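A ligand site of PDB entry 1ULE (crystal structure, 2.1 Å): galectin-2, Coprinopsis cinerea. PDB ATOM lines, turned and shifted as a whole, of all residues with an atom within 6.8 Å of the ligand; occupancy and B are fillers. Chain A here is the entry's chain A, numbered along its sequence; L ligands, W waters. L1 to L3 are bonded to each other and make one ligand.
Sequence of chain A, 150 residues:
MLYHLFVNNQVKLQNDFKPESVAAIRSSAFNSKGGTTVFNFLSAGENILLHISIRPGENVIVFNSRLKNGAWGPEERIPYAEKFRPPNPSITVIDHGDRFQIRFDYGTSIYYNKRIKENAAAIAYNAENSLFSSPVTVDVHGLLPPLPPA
Water W5 bridges O3 of LG3 L3 and NH2 of Arg 66.
Water W6 lies within hydrogen-bond range of an oxygen (O6) of LIG L1 (2.6 Å) and the side-chain carboxylate (OE1) of Glu 75 (2.7 Å).
Water W2 lies within hydrogen-bond range of N1 of LIG L1 (2.6 Å), OE2 of Glu 58 (2.7 Å) and NH2 of Arg 77 (3.3 Å).
Water W1 bridges the side-chain hydroxyl (OG) of Ser 53 and an oxygen (O3) of LG2 L2.
Water W7 bridges an oxygen (O1) of LG3 L3 and the side-chain amide nitrogen (ND2) of Asn 126.
The side-chain carboxylate (OE2) of Glu 75 is in salt-bridge range of the guanidinium group (NH2) of Arg 55 (3.9 Å).
OE1 of Glu 75 lies within salt-bridge range of NH2 of Arg 77 (2.7 Å).
The backbone carbonyl oxygen (O) of Asn 64 lies within hydrogen-bond range of the backbone NH (N) of His 51.
The guanidinium group (NH1) of Arg 55 lies within salt-bridge range of the side-chain carboxylate (OE1) of Glu 58 (3.3 Å).
The side-chain amide nitrogen (ND2) of Asn 64 sits at hydrogen-bond distance from the backbone carbonyl oxygen (O) of Gly 73 (2.8 Å).
The side-chain amide oxygen of Asn 64 sits close to the backbone carbonyl oxygen of Pro 74 (3.5 Å).
The backbone carbonyl oxygen (O) of Val 62 lies within hydrogen-bond range of the backbone NH (N) of Ser 53.
N of Asn 126 is in hydrogen-bond range of O of Val 38.
An oxygen (O5) of LG2 L2 is in hydrogen-bond range of the side-chain carboxylate (OE2) of Glu 75, 2.6 Å away.
A ring nitrogen (NE2) of His 51 is in hydrogen-bond range of an oxygen (O3) of LG2 L2, at 2.7 Å.
The guanidinium group (NH1) of Arg 55 lies within hydrogen-bond range of an oxygen (O2) of LIG L1.
The side-chain amide nitrogen (ND2) of Asn 64 is in hydrogen-bond range of an oxygen (O5) of LG2 L2 (2.9 Å).
The indole nitrogen (NE1) of Trp 72 lies within hydrogen-bond range of an oxygen (O5) of LG3 L3, at 3.1 Å.
O2 of LIG L1 lies close to NH2 of Arg 77, at 3.1 Å.
Residues that only touch the ligand: Val 38 and Ser 53.
Hydrophobic or aromatic side chains within 4 Å of the ligand: Val 38, His 51 and Trp 72.
Eight residues have an atom within 4 Å of the ligand: Val 38, His 51, Ser 53, Arg 55, Asn 64, Trp 72, Glu 75 and Arg 77.
The nearest printed residue that does not touch the ligand is Val 62 (4.01 Å).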
ATOM      1  N   THR A  36      14.575  -0.127   2.760  1.00  0.00           N
ATOM      2  CA  THR A  36      14.441   1.079   3.557  1.00  0.00           C
ATOM      3  C   THR A  36      14.947   2.285   2.774  1.00  0.00           C
ATOM      4  O   THR A  36      16.030   2.279   2.195  1.00  0.00           O
ATOM      5  CB  THR A  36      15.222   0.934   4.887  1.00  0.00           C
ATOM      6  OG1 THR A  36      14.574  -0.052   5.692  1.00  0.00           O
ATOM      7  CG2 THR A  36      15.269   2.254   5.641  1.00  0.00           C
ATOM      8  N   VAL A  38      15.421   6.524   2.983  1.00  0.00           N
ATOM      9  CA  VAL A  38      15.527   7.658   3.887  1.00  0.00           C
ATOM     10  C   VAL A  38      15.631   9.031   3.221  1.00  0.00           C
ATOM     11  O   VAL A  38      16.251   9.178   2.176  1.00  0.00           O
ATOM     12  CB  VAL A  38      16.778   7.479   4.802  1.00  0.00           C
ATOM     13  CG1 VAL A  38      17.033   8.746   5.596  1.00  0.00           C
ATOM     14  CG2 VAL A  38      16.572   6.293   5.731  1.00  0.00           C
ATOM     15  N   ASN A  40      16.399  13.062   4.590  1.00  0.00           N
ATOM     16  CA  ASN A  40      16.810  13.896   5.721  1.00  0.00           C
ATOM     17  C   ASN A  40      16.805  15.362   5.359  1.00  0.00           C
ATOM     18  O   ASN A  40      17.199  15.732   4.262  1.00  0.00           O
ATOM     19  CB  ASN A  40      18.254  13.591   6.171  1.00  0.00           C
ATOM     20  CG  ASN A  40      18.411  12.219   6.808  1.00  0.00           C
ATOM     21  OD1 ASN A  40      17.554  11.776   7.566  1.00  0.00           O
ATOM     22  ND2 ASN A  40      19.528  11.566   6.523  1.00  0.00           N
ATOM     23  N   HIS A  51      14.419  13.375  10.108  1.00  0.00           N
ATOM     24  CA  HIS A  51      14.828  12.110   9.522  1.00  0.00           C
ATOM     25  C   HIS A  51      13.555  11.304   9.267  1.00  0.00           C
ATOM     26  O   HIS A  51      12.748  11.089  10.176  1.00  0.00           O
ATOM     27  CB  HIS A  51      15.730  11.384  10.520  1.00  0.00           C
ATOM     28  CG  HIS A  51      16.074   9.971  10.139  1.00  0.00           C
ATOM     29  ND1 HIS A  51      16.922   9.663   9.108  1.00  0.00           N
ATOM     30  CD2 HIS A  51      15.717   8.792  10.700  1.00  0.00           C
ATOM     31  CE1 HIS A  51      17.083   8.353   9.047  1.00  0.00           C
ATOM     32  NE2 HIS A  51      16.355   7.798  10.013  1.00  0.00           N
ATOM     33  N   ILE A  52      13.348  10.890   8.015  1.00  0.00           N
ATOM     34  CA  ILE A  52      12.188  10.103   7.640  1.00  0.00           C
ATOM     35  C   ILE A  52      12.695   8.763   7.100  1.00  0.00           C
ATOM     36  O   ILE A  52      13.202   8.707   5.978  1.00  0.00           O
ATOM     37  CB  ILE A  52      11.354  10.793   6.536  1.00  0.00           C
ATOM     38  CG1 ILE A  52      10.952  12.201   6.973  1.00  0.00           C
ATOM     39  CG2 ILE A  52      10.096   9.979   6.248  1.00  0.00           C
ATOM     40  CD1 ILE A  52      10.252  13.004   5.889  1.00  0.00           C
ATOM     41  N   SER A  53      12.535   7.711   7.902  1.00  0.00           N
ATOM     42  CA  SER A  53      12.988   6.372   7.529  1.00  0.00           C
ATOM     43  C   SER A  53      11.810   5.485   7.137  1.00  0.00           C
ATOM     44  O   SER A  53      11.059   5.013   7.986  1.00  0.00           O
ATOM     45  CB  SER A  53      13.735   5.722   8.711  1.00  0.00           C
ATOM     46  OG  SER A  53      14.306   4.490   8.331  1.00  0.00           O
ATOM     47  N   ARG A  55      10.448   2.146   6.052  1.00  0.00           N
ATOM     48  CA  ARG A  55      10.838   0.729   6.093  1.00  0.00           C
ATOM     49  C   ARG A  55       9.692  -0.210   5.730  1.00  0.00           C
ATOM     50  O   ARG A  55       8.877  -0.565   6.582  1.00  0.00           O
ATOM     51  CB  ARG A  55      11.349   0.392   7.494  1.00  0.00           C
ATOM     52  CG  ARG A  55      12.329   1.415   8.053  1.00  0.00           C
ATOM     53  CD  ARG A  55      12.698   1.122   9.492  1.00  0.00           C
ATOM     54  NE  ARG A  55      13.465   2.219  10.092  1.00  0.00           N
ATOM     55  CZ  ARG A  55      13.837   2.254  11.364  1.00  0.00           C
ATOM     56  NH1 ARG A  55      13.538   1.256  12.182  1.00  0.00           N
ATOM     57  NH2 ARG A  55      14.517   3.301  11.824  1.00  0.00           N
ATOM     58  N   GLU A  58       9.683  -3.649   7.694  1.00  0.00           N
ATOM     59  CA  GLU A  58       9.289  -3.583   9.098  1.00  0.00           C
ATOM     60  C   GLU A  58       7.885  -2.978   9.176  1.00  0.00           C
ATOM     61  O   GLU A  58       7.343  -2.787  10.271  1.00  0.00           O
ATOM     62  CB  GLU A  58      10.307  -2.709   9.849  1.00  0.00           C
ATOM     63  CG  GLU A  58      10.307  -2.837  11.367  1.00  0.00           C
ATOM     64  CD  GLU A  58      11.328  -1.903  12.028  1.00  0.00           C
ATOM     65  OE1 GLU A  58      12.427  -1.727  11.458  1.00  0.00           O
ATOM     66  OE2 GLU A  58      11.031  -1.370  13.115  1.00  0.00           O
ATOM     67  N   VAL A  62       9.675   5.727  10.244  1.00  0.00           N
ATOM     68  CA  VAL A  62      10.191   6.313  11.469  1.00  0.00           C
ATOM     69  C   VAL A  62      10.677   7.752  11.316  1.00  0.00           C
ATOM     70  O   VAL A  62      11.346   8.092  10.344  1.00  0.00           O
ATOM     71  CB  VAL A  62      11.333   5.434  12.026  1.00  0.00           C
ATOM     72  CG1 VAL A  62      11.814   5.982  13.365  1.00  0.00           C
ATOM     73  CG2 VAL A  62      10.854   3.997  12.166  1.00  0.00           C
ATOM     74  N   PHE A  63      10.343   8.583  12.300  1.00  0.00           N
ATOM     75  CA  PHE A  63      10.744   9.982  12.315  1.00  0.00           C
ATOM     76  C   PHE A  63      11.644  10.221  13.528  1.00  0.00           C
ATOM     77  O   PHE A  63      11.360   9.716  14.613  1.00  0.00           O
ATOM     78  CB  PHE A  63       9.529  10.902  12.390  1.00  0.00           C
ATOM     79  CG  PHE A  63       8.542  10.713  11.265  1.00  0.00           C
ATOM     80  CD1 PHE A  63       7.577   9.705  11.320  1.00  0.00           C
ATOM     81  CD2 PHE A  63       8.609  11.519  10.128  1.00  0.00           C
ATOM     82  CE1 PHE A  63       6.684   9.515  10.267  1.00  0.00           C
ATOM     83  CE2 PHE A  63       7.715  11.328   9.074  1.00  0.00           C
ATOM     84  CZ  PHE A  63       6.753  10.321   9.139  1.00  0.00           C
ATOM     85  N   ASN A  64      12.707  10.993  13.350  1.00  0.00           N
ATOM     86  CA  ASN A  64      13.645  11.281  14.435  1.00  0.00           C
ATOM     87  C   ASN A  64      14.524  12.472  14.041  1.00  0.00           C
ATOM     88  O   ASN A  64      14.360  13.056  12.969  1.00  0.00           O
ATOM     89  CB  ASN A  64      14.532  10.058  14.703  1.00  0.00           C
ATOM     90  CG  ASN A  64      14.955   9.937  16.164  1.00  0.00           C
ATOM     91  OD1 ASN A  64      15.090  10.937  16.868  1.00  0.00           O
ATOM     92  ND2 ASN A  64      15.191   8.707  16.604  1.00  0.00           N
ATOM     93  N   SER A  65      15.472  12.808  14.923  1.00  0.00           N
ATOM     94  CA  SER A  65      16.415  13.908  14.678  1.00  0.00           C
ATOM     95  C   SER A  65      17.708  13.569  15.414  1.00  0.00           C
ATOM     96  O   SER A  65      17.729  12.686  16.271  1.00  0.00           O
ATOM     97  CB  SER A  65      15.880  15.230  15.257  1.00  0.00           C
ATOM     98  OG  SER A  65      14.609  15.583  14.742  1.00  0.00           O
ATOM     99  N   ARG A  66      18.795  14.259  15.074  1.00  0.00           N
ATOM    100  CA  ARG A  66      20.059  14.056  15.762  1.00  0.00           C
ATOM    101  C   ARG A  66      21.098  15.061  15.288  1.00  0.00           C
ATOM    102  O   ARG A  66      21.101  15.462  14.123  1.00  0.00           O
ATOM    103  CB  ARG A  66      20.588  12.620  15.577  1.00  0.00           C
ATOM    104  CG  ARG A  66      21.416  12.372  14.328  1.00  0.00           C
ATOM    105  CD  ARG A  66      22.099  10.999  14.391  1.00  0.00           C
ATOM    106  NE  ARG A  66      22.760  10.650  13.129  1.00  0.00           N
ATOM    107  CZ  ARG A  66      23.945  11.107  12.748  1.00  0.00           C
ATOM    108  NH1 ARG A  66      24.619  11.933  13.520  1.00  0.00           N
ATOM    109  NH2 ARG A  66      24.448  10.756  11.574  1.00  0.00           N
ATOM    110  N   TRP A  72      20.723   9.502  18.116  1.00  0.00           N
ATOM    111  CA  TRP A  72      19.325   9.593  17.738  1.00  0.00           C
ATOM    112  C   TRP A  72      18.511   9.877  19.000  1.00  0.00           C
ATOM    113  O   TRP A  72      18.902   9.495  20.093  1.00  0.00           O
ATOM    114  CB  TRP A  72      18.833   8.273  17.127  1.00  0.00           C
ATOM    115  CG  TRP A  72      19.378   8.001  15.750  1.00  0.00           C
ATOM    116  CD1 TRP A  72      20.249   7.013  15.390  1.00  0.00           C
ATOM    117  CD2 TRP A  72      19.124   8.764  14.568  1.00  0.00           C
ATOM    118  NE1 TRP A  72      20.557   7.122  14.051  1.00  0.00           N
ATOM    119  CE2 TRP A  72      19.883   8.190  13.522  1.00  0.00           C
ATOM    120  CE3 TRP A  72      18.335   9.890  14.276  1.00  0.00           C
ATOM    121  CZ2 TRP A  72      19.876   8.687  12.216  1.00  0.00           C
ATOM    122  CZ3 TRP A  72      18.318  10.394  12.982  1.00  0.00           C
ATOM    123  CH2 TRP A  72      19.092   9.794  11.967  1.00  0.00           C
ATOM    124  N   GLY A  73      17.370  10.551  18.845  1.00  0.00           N
ATOM    125  CA  GLY A  73      16.530  10.823  19.992  1.00  0.00           C
ATOM    126  C   GLY A  73      15.457   9.751  20.016  1.00  0.00           C
ATOM    127  O   GLY A  73      15.626   8.707  19.401  1.00  0.00           O
ATOM    128  N   PRO A  74      14.342   9.961  20.737  1.00  0.00           N
ATOM    129  CA  PRO A  74      13.267   8.962  20.785  1.00  0.00           C
ATOM    130  C   PRO A  74      12.534   8.924  19.443  1.00  0.00           C
ATOM    131  O   PRO A  74      12.383   9.963  18.796  1.00  0.00           O
ATOM    132  CB  PRO A  74      12.386   9.452  21.929  1.00  0.00           C
ATOM    133  CG  PRO A  74      12.585  10.946  21.889  1.00  0.00           C
ATOM    134  CD  PRO A  74      14.073  11.060  21.679  1.00  0.00           C
ATOM    135  N   GLU A  75      12.093   7.750  19.022  1.00  0.00           N
ATOM    136  CA  GLU A  75      11.416   7.605  17.739  1.00  0.00           C
ATOM    137  C   GLU A  75       9.923   7.891  17.786  1.00  0.00           C
ATOM    138  O   GLU A  75       9.268   7.734  18.809  1.00  0.00           O
ATOM    139  CB  GLU A  75      11.617   6.196  17.184  1.00  0.00           C
ATOM    140  CG  GLU A  75      13.066   5.758  17.007  1.00  0.00           C
ATOM    141  CD  GLU A  75      13.192   4.397  16.341  1.00  0.00           C
ATOM    142  OE1 GLU A  75      12.335   3.531  16.594  1.00  0.00           O
ATOM    143  OE2 GLU A  75      14.163   4.196  15.570  1.00  0.00           O
ATOM    144  N   GLU A  76       9.405   8.338  16.644  1.00  0.00           N
ATOM    145  CA  GLU A  76       7.988   8.608  16.470  1.00  0.00           C
ATOM    146  C   GLU A  76       7.654   7.762  15.250  1.00  0.00           C
ATOM    147  O   GLU A  76       8.264   7.925  14.185  1.00  0.00           O
ATOM    148  CB  GLU A  76       7.738  10.102  16.265  1.00  0.00           C
ATOM    149  CG  GLU A  76       7.970  10.889  17.566  1.00  0.00           C
ATOM    150  CD  GLU A  76       7.817  12.403  17.429  1.00  0.00           C
ATOM    151  OE1 GLU A  76       6.818  12.854  16.831  1.00  0.00           O
ATOM    152  OE2 GLU A  76       8.693  13.144  17.937  1.00  0.00           O
ATOM    153  N   ARG A  77       6.711   6.847  15.404  1.00  0.00           N
ATOM    154  CA  ARG A  77       6.356   5.916  14.341  1.00  0.00           C
ATOM    155  C   ARG A  77       4.911   5.918  13.850  1.00  0.00           C
ATOM    156  O   ARG A  77       4.002   6.384  14.528  1.00  0.00           O
ATOM    157  CB  ARG A  77       6.688   4.496  14.778  1.00  0.00           C
ATOM    158  CG  ARG A  77       8.137   4.263  15.158  1.00  0.00           C
ATOM    159  CD  ARG A  77       8.316   2.899  15.810  1.00  0.00           C
ATOM    160  NE  ARG A  77       9.722   2.530  15.914  1.00  0.00           N
ATOM    161  CZ  ARG A  77      10.261   1.468  15.309  1.00  0.00           C
ATOM    162  NH1 ARG A  77       9.503   0.671  14.573  1.00  0.00           N
ATOM    163  NH2 ARG A  77      11.552   1.223  15.437  1.00  0.00           N
ATOM    164  N   ASN A 126      18.754   8.790   0.875  1.00  0.00           N
ATOM    165  CA  ASN A 126      19.630   7.620   0.955  1.00  0.00           C
ATOM    166  C   ASN A 126      18.887   6.285   0.847  1.00  0.00           C
ATOM    167  O   ASN A 126      17.795   6.131   1.382  1.00  0.00           O
ATOM    168  CB  ASN A 126      20.419   7.622   2.268  1.00  0.00           C
ATOM    169  CG  ASN A 126      21.202   8.898   2.465  1.00  0.00           C
ATOM    170  OD1 ASN A 126      22.013   9.273   1.622  1.00  0.00           O
ATOM    171  ND2 ASN A 126      20.959   9.573   3.588  1.00  0.00           N
HETATM  172  C1  LIG L   1      16.497  -0.235  17.351  1.00  0.00           C
HETATM  173  C2  LIG L   1      15.314   0.549  16.782  1.00  0.00           C
HETATM  174  C3  LIG L   1      15.637   0.929  15.340  1.00  0.00           C
HETATM  175  C4  LIG L   1      16.944   1.714  15.290  1.00  0.00           C
HETATM  176  C5  LIG L   1      18.067   0.917  15.987  1.00  0.00           C
HETATM  177  C6  LIG L   1      19.389   1.670  16.082  1.00  0.00           C
HETATM  178  C7  LIG L   1      13.209  -0.041  17.811  1.00  0.00           C
HETATM  179  C8  LIG L   1      11.898  -0.821  17.727  1.00  0.00           C
HETATM  180  N1  LIG L   1      14.099  -0.251  16.843  1.00  0.00           N
HETATM  181  O1  LIG L   1      16.234  -0.560  18.671  1.00  0.00           O
HETATM  182  O2  LIG L   1      14.587   1.709  14.782  1.00  0.00           O
HETATM  183  O3  LIG L   1      17.297   1.938  13.918  1.00  0.00           O
HETATM  184  O4  LIG L   1      17.672   0.586  17.328  1.00  0.00           O
HETATM  185  O5  LIG L   1      19.222   2.953  16.672  1.00  0.00           O
HETATM  186  O6  LIG L   1      13.394   0.752  18.731  1.00  0.00           O
HETATM  187  C1  LG2 L   2      17.771   3.202  13.610  1.00  0.00           C
HETATM  188  C2  LG2 L   2      18.326   3.171  12.207  1.00  0.00           C
HETATM  189  C3  LG2 L   2      18.797   4.567  11.825  1.00  0.00           C
HETATM  190  C4  LG2 L   2      17.662   5.586  11.985  1.00  0.00           C
HETATM  191  C5  LG2 L   2      17.095   5.489  13.414  1.00  0.00           C
HETATM  192  C6  LG2 L   2      15.892   6.375  13.623  1.00  0.00           C
HETATM  193  O1  LG2 L   2      19.418   2.258  12.160  1.00  0.00           O
HETATM  194  O2  LG2 L   2      19.259   4.563  10.461  1.00  0.00           O
HETATM  195  O3  LG2 L   2      16.633   5.329  11.041  1.00  0.00           O
HETATM  196  O4  LG2 L   2      16.685   4.128  13.696  1.00  0.00           O
HETATM  197  O5  LG2 L   2      15.466   6.327  14.984  1.00  0.00           O
HETATM  198  C1  LG3 L   3      20.159   5.585  10.131  1.00  0.00           C
HETATM  199  C2  LG3 L   3      20.678   5.366   8.713  1.00  0.00           C
HETATM  200  C3  LG3 L   3      21.584   4.139   8.678  1.00  0.00           C
HETATM  201  C4  LG3 L   3      22.706   4.291   9.704  1.00  0.00           C
HETATM  202  C5  LG3 L   3      22.108   4.537  11.095  1.00  0.00           C
HETATM  203  C6  LG3 L   3      23.165   4.796  12.156  1.00  0.00           C
HETATM  204  O1  LG3 L   3      19.577   5.163   7.832  1.00  0.00           O
HETATM  205  O2  LG3 L   3      22.134   3.996   7.380  1.00  0.00           O
HETATM  206  O3  LG3 L   3      23.535   5.385   9.341  1.00  0.00           O
HETATM  207  O4  LG3 L   3      21.237   5.689  11.057  1.00  0.00           O
HETATM  208  O5  LG3 L   3      22.569   4.905  13.447  1.00  0.00           O
HETATM  209  O   HOH W   1      16.870   3.974   8.616  1.00  0.00           O
HETATM  210  O   HOH W   2      13.271  -1.470  14.671  1.00  0.00           O
HETATM  211  O   HOH W   3      26.398   4.434   9.601  1.00  0.00           O
HETATM  212  O   HOH W   4      19.858   4.673   5.033  1.00  0.00           O
HETATM  213  O   HOH W   5      24.216   7.860   9.834  1.00  0.00           O
HETATM  214  O   HOH W   6      11.782   2.786  19.105  1.00  0.00           O
HETATM  215  O   HOH W   7      20.491   7.121   5.725  1.00  0.00           O
HETATM  216  O   HOH W   8      21.997   2.080  13.408  1.00  0.00           O
HETATM  217  O   HOH W   9      23.508   6.596   6.175  1.00  0.00           O
HETATM  218  O   HOH W  10      17.221   5.073  17.087  1.00  0.00           O
HETATM  219  O   HOH W  11      17.583   1.371  20.446  1.00  0.00           O
